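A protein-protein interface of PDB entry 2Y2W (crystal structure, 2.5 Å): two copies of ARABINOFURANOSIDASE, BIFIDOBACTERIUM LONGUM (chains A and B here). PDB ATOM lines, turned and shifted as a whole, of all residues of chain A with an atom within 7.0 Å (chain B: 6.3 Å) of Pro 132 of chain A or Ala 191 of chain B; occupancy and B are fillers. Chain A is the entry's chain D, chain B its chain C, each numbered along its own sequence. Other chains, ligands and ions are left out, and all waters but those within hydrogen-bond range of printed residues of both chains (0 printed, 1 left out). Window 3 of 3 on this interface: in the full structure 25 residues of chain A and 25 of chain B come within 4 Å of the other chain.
The backbone carbonyl oxygen of Met 133 of chain A is in hydrogen-bond range of the side-chain hydroxyl of Thr 190 of chain B (3.1 Å). The backbone carbonyl oxygen of Met 133 of chain A is in hydrogen-bond range of the backbone NH of Ala 191 of chain B, 2.8 Å away.
The side-chain carboxylate (OD2) of Asp 123 of chain A lies within salt-bridge range of the guanidinium group (NE) of Arg 134 of chain A, 2.8 Å away. The side-chain amide nitrogen (ND2) of Asn 145 of chain A is in hydrogen-bond range of the backbone carbonyl oxygen (O) of Pro 132 of chain A, at 2.9 Å. The backbone NH of Gly 189 of chain B sits at hydrogen-bond distance from the side-chain carboxylate of Asp 194 of chain B (2.9 Å). The side-chain hydroxyl (OG1) of Thr 190 of chain B lies within hydrogen-bond range of the side-chain carboxylate (OE2) of Glu 182 of chain B (2.7 Å). N of Glu 143 of chain A is in hydrogen-bond range of O of Arg 134 of chain A, at 2.6 Å.
Pro 132 of chain A touches Ala 191 of chain B. Gly 189 of chain B touches Met 133 of chain A (O to CE, 3.3 Å). Arg 134 of chain A touches Thr 190 of chain B (CA to OG1, 3.7 Å). Arg 134 of chain A touches Ala 191 of chain B (NH1 to CB, 3.5 Å). NH1 of Arg 134 of chain A touches NE1 of Trp 192 of chain B, at 3.7 Å. OE1 of Glu 182 of chain B touches CD of Arg 135 of chain A (3.5 Å). N of Arg 135 of chain A touches OG1 of Thr 190 of chain B, 3.9 Å away.
Of the printed residues of chain B, Pro 132 of chain A touches Ala 191. Of the printed residues of chain B, Met 133 of chain A touches Gly 189 (3.3 Å), Thr 190 (3.1 Å) and Ala 191 (2.8 Å). Printed residues of chain A within 4 Å of Gly 189 of chain B: Met 133 (3.3 Å). Printed residues of chain A within 4 Å of Thr 190 of chain B: Met 133 (3.1 Å), Arg 134 (3.7 Å) and Arg 135 (3.9 Å). Ala 191 of chain B touches just these residues of chain A: Pro 132, Met 133 and Arg 134. Printed residues of chain A within 4 Å of Trp 192 of chain B: Arg 134. Arg 196 of chain B touches none of the printed residues of chain A. The nearest printed residue of chain B that does not touch Pro 132 of chain A is Thr 190 of chain B (6.6 Å). The nearest residue of chain A that does not touch Ala 191 of chain B is Arg 135 of chain A (6.6 Å).
Along chain B the printed residues that touch a printed residue of chain A span positions 182 to 192. Of the 17 printed residues of chain A, 4 touch a printed residue of chain B. Hydrophobic or aromatic side chains of chain A that line the printed part of chain B: Pro 132 and Met 133. Among the printed residues, no Asp or Glu carboxylate lies within 4 Å of a Lys or Arg side-chain nitrogen of the other chain.
No position is printed for both chains.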
ATOM      1  N   GLU A 122      28.939  16.490 -14.362  1.00  0.00           N
ATOM      2  CA  GLU A 122      28.079  17.087 -15.391  1.00  0.00           C
ATOM      3  C   GLU A 122      27.516  18.439 -14.960  1.00  0.00           C
ATOM      4  O   GLU A 122      27.106  19.242 -15.803  1.00  0.00           O
ATOM      5  CB  GLU A 122      26.910  16.163 -15.758  1.00  0.00           C
ATOM      6  CG  GLU A 122      27.279  14.717 -16.051  1.00  0.00           C
ATOM      7  CD  GLU A 122      27.218  13.834 -14.813  1.00  0.00           C
ATOM      8  OE1 GLU A 122      27.644  14.282 -13.726  1.00  0.00           O
ATOM      9  OE2 GLU A 122      26.747  12.682 -14.930  1.00  0.00           O
ATOM     10  N   ASP A 123      27.484  18.680 -13.651  1.00  0.00           N
ATOM     11  CA  ASP A 123      27.004  19.951 -13.103  1.00  0.00           C
ATOM     12  C   ASP A 123      27.885  21.128 -13.508  1.00  0.00           C
ATOM     13  O   ASP A 123      27.441  22.277 -13.480  1.00  0.00           O
ATOM     14  CB  ASP A 123      26.907  19.884 -11.574  1.00  0.00           C
ATOM     15  CG  ASP A 123      25.756  19.022 -11.095  1.00  0.00           C
ATOM     16  OD1 ASP A 123      24.832  18.748 -11.891  1.00  0.00           O
ATOM     17  OD2 ASP A 123      25.771  18.628  -9.910  1.00  0.00           O
ATOM     18  N   GLY A 124      29.128  20.831 -13.881  1.00  0.00           N
ATOM     19  CA  GLY A 124      30.101  21.859 -14.232  1.00  0.00           C
ATOM     20  C   GLY A 124      30.399  21.975 -15.715  1.00  0.00           C
ATOM     21  O   GLY A 124      31.336  22.668 -16.105  1.00  0.00           O
ATOM     22  N   ILE A 125      29.612  21.288 -16.541  1.00  0.00           N
ATOM     23  CA  ILE A 125      29.766  21.355 -17.999  1.00  0.00           C
ATOM     24  C   ILE A 125      28.588  22.087 -18.643  1.00  0.00           C
ATOM     25  O   ILE A 125      27.566  22.338 -17.995  1.00  0.00           O
ATOM     26  CB  ILE A 125      29.948  19.947 -18.655  1.00  0.00           C
ATOM     27  CG1 ILE A 125      28.672  19.104 -18.525  1.00  0.00           C
ATOM     28  CG2 ILE A 125      31.162  19.233 -18.074  1.00  0.00           C
ATOM     29  CD1 ILE A 125      28.618  17.901 -19.442  1.00  0.00           C
ATOM     30  N   PRO A 127      26.671  25.348 -20.826  1.00  0.00           N
ATOM     31  CA  PRO A 127      26.557  26.795 -20.614  1.00  0.00           C
ATOM     32  C   PRO A 127      26.360  27.145 -19.137  1.00  0.00           C
ATOM     33  O   PRO A 127      25.482  26.576 -18.482  1.00  0.00           O
ATOM     34  CB  PRO A 127      25.310  27.175 -21.429  1.00  0.00           C
ATOM     35  CG  PRO A 127      25.109  26.036 -22.393  1.00  0.00           C
ATOM     36  CD  PRO A 127      25.563  24.826 -21.648  1.00  0.00           C
ATOM     37  N   ARG A 128      27.178  28.072 -18.629  1.00  0.00           N
ATOM     38  CA  ARG A 128      27.115  28.509 -17.226  1.00  0.00           C
ATOM     39  C   ARG A 128      25.701  28.850 -16.768  1.00  0.00           C
ATOM     40  O   ARG A 128      25.283  28.452 -15.678  1.00  0.00           O
ATOM     41  CB  ARG A 128      28.020  29.716 -16.986  1.00  0.00           C
ATOM     42  CG  ARG A 128      29.481  29.384 -16.797  1.00  0.00           C
ATOM     43  CD  ARG A 128      30.236  30.591 -16.276  1.00  0.00           C
ATOM     44  NE  ARG A 128      31.678  30.453 -16.456  1.00  0.00           N
ATOM     45  CZ  ARG A 128      32.350  30.885 -17.520  1.00  0.00           C
ATOM     46  NH1 ARG A 128      31.719  31.491 -18.518  1.00  0.00           N
ATOM     47  NH2 ARG A 128      33.660  30.712 -17.585  1.00  0.00           N
ATOM     48  N   GLU A 129      24.978  29.585 -17.612  1.00  0.00           N
ATOM     49  CA  GLU A 129      23.607  30.013 -17.325  1.00  0.00           C
ATOM     50  C   GLU A 129      22.758  28.881 -16.759  1.00  0.00           C
ATOM     51  O   GLU A 129      22.002  29.080 -15.807  1.00  0.00           O
ATOM     52  CB  GLU A 129      22.933  30.571 -18.586  1.00  0.00           C
ATOM     53  CG  GLU A 129      23.619  31.788 -19.206  1.00  0.00           C
ATOM     54  CD  GLU A 129      24.846  31.427 -20.036  1.00  0.00           C
ATOM     55  OE1 GLU A 129      24.808  30.393 -20.743  1.00  0.00           O
ATOM     56  OE2 GLU A 129      25.843  32.184 -19.985  1.00  0.00           O
ATOM     57  N   ASN A 130      22.915  27.692 -17.337  1.00  0.00           N
ATOM     58  CA  ASN A 130      22.041  26.559 -17.050  1.00  0.00           C
ATOM     59  C   ASN A 130      22.634  25.514 -16.097  1.00  0.00           C
ATOM     60  O   ASN A 130      22.049  24.444 -15.898  1.00  0.00           O
ATOM     61  CB  ASN A 130      21.585  25.916 -18.369  1.00  0.00           C
ATOM     62  CG  ASN A 130      20.808  26.888 -19.255  1.00  0.00           C
ATOM     63  OD1 ASN A 130      21.343  27.426 -20.225  1.00  0.00           O
ATOM     64  ND2 ASN A 130      19.546  27.130 -18.909  1.00  0.00           N
ATOM     65  N   ARG A 131      23.780  25.835 -15.498  1.00  0.00           N
ATOM     66  CA  ARG A 131      24.407  24.947 -14.517  1.00  0.00           C
ATOM     67  C   ARG A 131      23.730  25.076 -13.149  1.00  0.00           C
ATOM     68  O   ARG A 131      23.501  26.190 -12.675  1.00  0.00           O
ATOM     69  CB  ARG A 131      25.909  25.225 -14.402  1.00  0.00           C
ATOM     70  CG  ARG A 131      26.688  25.000 -15.691  1.00  0.00           C
ATOM     71  CD  ARG A 131      28.172  25.220 -15.480  1.00  0.00           C
ATOM     72  NE  ARG A 131      28.880  25.460 -16.737  1.00  0.00           N
ATOM     73  CZ  ARG A 131      30.200  25.601 -16.845  1.00  0.00           C
ATOM     74  NH1 ARG A 131      30.981  25.525 -15.771  1.00  0.00           N
ATOM     75  NH2 ARG A 131      30.743  25.818 -18.032  1.00  0.00           N
ATOM     76  N   PRO A 132      23.403  23.934 -12.512  1.00  0.00           N
ATOM     77  CA  PRO A 132      22.698  23.957 -11.229  1.00  0.00           C
ATOM     78  C   PRO A 132      23.585  24.410 -10.070  1.00  0.00           C
ATOM     79  O   PRO A 132      24.801  24.198 -10.092  1.00  0.00           O
ATOM     80  CB  PRO A 132      22.282  22.497 -11.035  1.00  0.00           C
ATOM     81  CG  PRO A 132      23.304  21.721 -11.773  1.00  0.00           C
ATOM     82  CD  PRO A 132      23.671  22.555 -12.965  1.00  0.00           C
ATOM     83  N   MET A 133      22.970  25.035  -9.072  1.00  0.00           N
ATOM     84  CA  MET A 133      23.685  25.436  -7.874  1.00  0.00           C
ATOM     85  C   MET A 133      23.588  24.309  -6.848  1.00  0.00           C
ATOM     86  O   MET A 133      22.496  23.815  -6.551  1.00  0.00           O
ATOM     87  CB  MET A 133      23.137  26.758  -7.336  1.00  0.00           C
ATOM     88  CG  MET A 133      24.235  27.738  -6.956  1.00  0.00           C
ATOM     89  SD  MET A 133      23.837  29.465  -7.290  1.00  0.00           S
ATOM     90  CE  MET A 133      23.316  30.014  -5.663  1.00  0.00           C
ATOM     91  N   ARG A 134      24.740  23.898  -6.325  1.00  0.00           N
ATOM     92  CA  ARG A 134      24.844  22.665  -5.544  1.00  0.00           C
ATOM     93  C   ARG A 134      25.482  22.860  -4.173  1.00  0.00           C
ATOM     94  O   ARG A 134      26.143  23.869  -3.916  1.00  0.00           O
ATOM     95  CB  ARG A 134      25.633  21.610  -6.332  1.00  0.00           C
ATOM     96  CG  ARG A 134      24.937  21.097  -7.588  1.00  0.00           C
ATOM     97  CD  ARG A 134      23.973  19.962  -7.283  1.00  0.00           C
ATOM     98  NE  ARG A 134      23.493  19.335  -8.510  1.00  0.00           N
ATOM     99  CZ  ARG A 134      22.231  19.350  -8.928  1.00  0.00           C
ATOM    100  NH1 ARG A 134      21.285  19.947  -8.211  1.00  0.00           N
ATOM    101  NH2 ARG A 134      21.910  18.751 -10.067  1.00  0.00           N
ATOM    102  N   ARG A 135      25.265  21.881  -3.297  1.00  0.00           N
ATOM    103  CA  ARG A 135      25.893  21.834  -1.986  1.00  0.00           C
ATOM    104  C   ARG A 135      27.220  21.104  -2.077  1.00  0.00           C
ATOM    105  O   ARG A 135      27.357  20.145  -2.839  1.00  0.00           O
ATOM    106  CB  ARG A 135      25.014  21.052  -1.010  1.00  0.00           C
ATOM    107  CG  ARG A 135      23.893  21.817  -0.358  1.00  0.00           C
ATOM    108  CD  ARG A 135      23.150  20.893   0.594  1.00  0.00           C
ATOM    109  NE  ARG A 135      22.355  21.624   1.575  1.00  0.00           N
ATOM    110  CZ  ARG A 135      21.667  21.059   2.561  1.00  0.00           C
ATOM    111  NH1 ARG A 135      21.660  19.736   2.711  1.00  0.00           N
ATOM    112  NH2 ARG A 135      20.978  21.820   3.402  1.00  0.00           N
ATOM    113  N   GLU A 143      27.961  25.750  -4.061  1.00  0.00           N
ATOM    114  CA  GLU A 143      28.793  25.802  -5.256  1.00  0.00           C
ATOM    115  C   GLU A 143      27.964  26.191  -6.486  1.00  0.00           C
ATOM    116  O   GLU A 143      26.989  25.518  -6.839  1.00  0.00           O
ATOM    117  CB  GLU A 143      29.482  24.445  -5.451  1.00  0.00           C
ATOM    118  CG  GLU A 143      30.091  24.199  -6.827  1.00  0.00           C
ATOM    119  CD  GLU A 143      31.456  24.829  -7.007  1.00  0.00           C
ATOM    120  OE1 GLU A 143      32.216  24.941  -6.021  1.00  0.00           O
ATOM    121  OE2 GLU A 143      31.779  25.198  -8.152  1.00  0.00           O
ATOM    122  N   THR A 144      28.366  27.282  -7.133  1.00  0.00           N
ATOM    123  CA  THR A 144      27.657  27.809  -8.297  1.00  0.00           C
ATOM    124  C   THR A 144      27.969  27.027  -9.565  1.00  0.00           C
ATOM    125  O   THR A 144      27.193  27.064 -10.526  1.00  0.00           O
ATOM    126  CB  THR A 144      27.992  29.289  -8.545  1.00  0.00           C
ATOM    127  OG1 THR A 144      29.406  29.431  -8.741  1.00  0.00           O
ATOM    128  CG2 THR A 144      27.553  30.140  -7.368  1.00  0.00           C
ATOM    129  N   ASN A 145      29.108  26.336  -9.558  1.00  0.00           N
ATOM    130  CA  ASN A 145      29.592  25.548 -10.697  1.00  0.00           C
ATOM    131  C   ASN A 145      29.970  26.379 -11.925  1.00  0.00           C
ATOM    132  O   ASN A 145      29.983  25.871 -13.048  1.00  0.00           O
ATOM    133  CB  ASN A 145      28.608  24.423 -11.061  1.00  0.00           C
ATOM    134  CG  ASN A 145      28.589  23.309 -10.034  1.00  0.00           C
ATOM    135  OD1 ASN A 145      29.596  22.633  -9.813  1.00  0.00           O
ATOM    136  ND2 ASN A 145      27.439  23.107  -9.403  1.00  0.00           N
ATOM    137  N   GLU A 146      30.294  27.651 -11.701  1.00  0.00           N
ATOM    138  CA  GLU A 146      30.820  28.519 -12.757  1.00  0.00           C
ATOM    139  C   GLU A 146      32.132  27.961 -13.304  1.00  0.00           C
ATOM    140  O   GLU A 146      32.465  28.168 -14.470  1.00  0.00           O
ATOM    141  CB  GLU A 146      31.019  29.945 -12.242  1.00  0.00           C
ATOM    142  CG  GLU A 146      29.721  30.691 -11.947  1.00  0.00           C
ATOM    143  CD  GLU A 146      29.936  31.940 -11.106  1.00  0.00           C
ATOM    144  OE1 GLU A 146      30.835  32.748 -11.436  1.00  0.00           O
ATOM    145  OE2 GLU A 146      29.194  32.119 -10.114  1.00  0.00           O
ATOM    146  N   GLU B 182      18.588  17.625   1.055  1.00  0.00           N
ATOM    147  CA  GLU B 182      18.744  18.979   0.523  1.00  0.00           C
ATOM    148  C   GLU B 182      17.411  19.575   0.054  1.00  0.00           C
ATOM    149  O   GLU B 182      17.112  20.739   0.338  1.00  0.00           O
ATOM    150  CB  GLU B 182      19.761  18.974  -0.624  1.00  0.00           C
ATOM    151  CG  GLU B 182      20.094  20.349  -1.199  1.00  0.00           C
ATOM    152  CD  GLU B 182      21.076  20.289  -2.364  1.00  0.00           C
ATOM    153  OE1 GLU B 182      21.996  19.436  -2.353  1.00  0.00           O
ATOM    154  OE2 GLU B 182      20.923  21.098  -3.299  1.00  0.00           O
ATOM    155  N   GLY B 189      18.040  28.723  -2.871  1.00  0.00           N
ATOM    156  CA  GLY B 189      19.311  29.106  -3.480  1.00  0.00           C
ATOM    157  C   GLY B 189      20.016  27.943  -4.147  1.00  0.00           C
ATOM    158  O   GLY B 189      20.628  28.101  -5.203  1.00  0.00           O
ATOM    159  N   THR B 190      19.941  26.775  -3.520  1.00  0.00           N
ATOM    160  CA  THR B 190      20.441  25.549  -4.122  1.00  0.00           C
ATOM    161  C   THR B 190      19.371  24.995  -5.076  1.00  0.00           C
ATOM    162  O   THR B 190      18.179  25.285  -4.912  1.00  0.00           O
ATOM    163  CB  THR B 190      20.857  24.529  -3.032  1.00  0.00           C
ATOM    164  OG1 THR B 190      21.817  23.610  -3.561  1.00  0.00           O
ATOM    165  CG2 THR B 190      19.660  23.767  -2.491  1.00  0.00           C
ATOM    166  N   ALA B 191      19.797  24.223  -6.073  1.00  0.00           N
ATOM    167  CA  ALA B 191      18.884  23.714  -7.107  1.00  0.00           C
ATOM    168  C   ALA B 191      17.787  22.771  -6.593  1.00  0.00           C
ATOM    169  O   ALA B 191      16.658  22.803  -7.092  1.00  0.00           O
ATOM    170  CB  ALA B 191      19.661  23.055  -8.230  1.00  0.00           C
ATOM    171  N   TRP B 192      18.116  21.941  -5.605  1.00  0.00           N
ATOM    172  CA  TRP B 192      17.139  21.019  -5.021  1.00  0.00           C
ATOM    173  C   TRP B 192      16.085  21.741  -4.185  1.00  0.00           C
ATOM    174  O   TRP B 192      14.902  21.395  -4.240  1.00  0.00           O
ATOM    175  CB  TRP B 192      17.823  19.934  -4.183  1.00  0.00           C
ATOM    176  CG  TRP B 192      18.432  18.822  -4.990  1.00  0.00           C
ATOM    177  CD1 TRP B 192      19.757  18.503  -5.072  1.00  0.00           C
ATOM    178  CD2 TRP B 192      17.740  17.882  -5.826  1.00  0.00           C
ATOM    179  NE1 TRP B 192      19.936  17.425  -5.905  1.00  0.00           N
ATOM    180  CE2 TRP B 192      18.716  17.023  -6.382  1.00  0.00           C
ATOM    181  CE3 TRP B 192      16.394  17.682  -6.161  1.00  0.00           C
ATOM    182  CZ2 TRP B 192      18.388  15.977  -7.255  1.00  0.00           C
ATOM    183  CZ3 TRP B 192      16.067  16.643  -7.031  1.00  0.00           C
ATOM    184  CH2 TRP B 192      17.064  15.804  -7.567  1.00  0.00           C
ATOM    185  N   ALA B 193      16.517  22.740  -3.415  1.00  0.00           N
ATOM    186  CA  ALA B 193      15.612  23.511  -2.565  1.00  0.00           C
ATOM    187  C   ALA B 193      14.704  24.433  -3.378  1.00  0.00           C
ATOM    188  O   ALA B 193      13.556  24.668  -2.995  1.00  0.00           O
ATOM    189  CB  ALA B 193      16.386  24.302  -1.533  1.00  0.00           C
ATOM    190  N   ASP B 194      15.223  24.945  -4.494  1.00  0.00           N
ATOM    191  CA  ASP B 194      14.434  25.766  -5.414  1.00  0.00           C
ATOM    192  C   ASP B 194      13.274  24.985  -6.027  1.00  0.00           C
ATOM    193  O   ASP B 194      12.214  25.552  -6.295  1.00  0.00           O
ATOM    194  CB  ASP B 194      15.316  26.358  -6.516  1.00  0.00           C
ATOM    195  CG  ASP B 194      16.143  27.537  -6.039  1.00  0.00           C
ATOM    196  OD1 ASP B 194      16.049  27.917  -4.850  1.00  0.00           O
ATOM    197  OD2 ASP B 194      16.894  28.095  -6.864  1.00  0.00           O
ATOM    198  N   GLN B 195      13.479  23.687  -6.243  1.00  0.00           N
ATOM    199  CA  GLN B 195      12.411  22.808  -6.719  1.00  0.00           C
ATOM    200  C   GLN B 195      11.260  22.750  -5.721  1.00  0.00           C
ATOM    201  O   GLN B 195      10.097  22.831  -6.116  1.00  0.00           O
ATOM    202  CB  GLN B 195      12.941  21.405  -7.033  1.00  0.00           C
ATOM    203  CG  GLN B 195      13.547  21.279  -8.429  1.00  0.00           C
ATOM    204  CD  GLN B 195      14.079  19.883  -8.744  1.00  0.00           C
ATOM    205  OE1 GLN B 195      15.165  19.739  -9.308  1.00  0.00           O
ATOM    206  NE2 GLN B 195      13.313  18.855  -8.390  1.00  0.00           N
ATOM    207  N   ARG B 196      11.592  22.644  -4.434  1.00  0.00           N
ATOM    208  CA  ARG B 196      10.588  22.628  -3.370  1.00  0.00           C
ATOM    209  C   ARG B 196       9.763  23.913  -3.350  1.00  0.00           C
ATOM    210  O   ARG B 196       8.533  23.865  -3.257  1.00  0.00           O
ATOM    211  CB  ARG B 196      11.240  22.410  -2.004  1.00  0.00           C
ATOM    212  CG  ARG B 196      10.251  22.036  -0.911  1.00  0.00           C
ATOM    213  CD  ARG B 196      10.558  22.730   0.405  1.00  0.00           C
ATOM    214  NE  ARG B 196      11.929  22.506   0.843  1.00  0.00           N
ATOM    215  CZ  ARG B 196      12.835  23.462   1.034  1.00  0.00           C
ATOM    216  NH1 ARG B 196      12.526  24.739   0.845  1.00  0.00           N
ATOM    217  NH2 ARG B 196      14.055  23.130   1.427  1.00  0.00           N
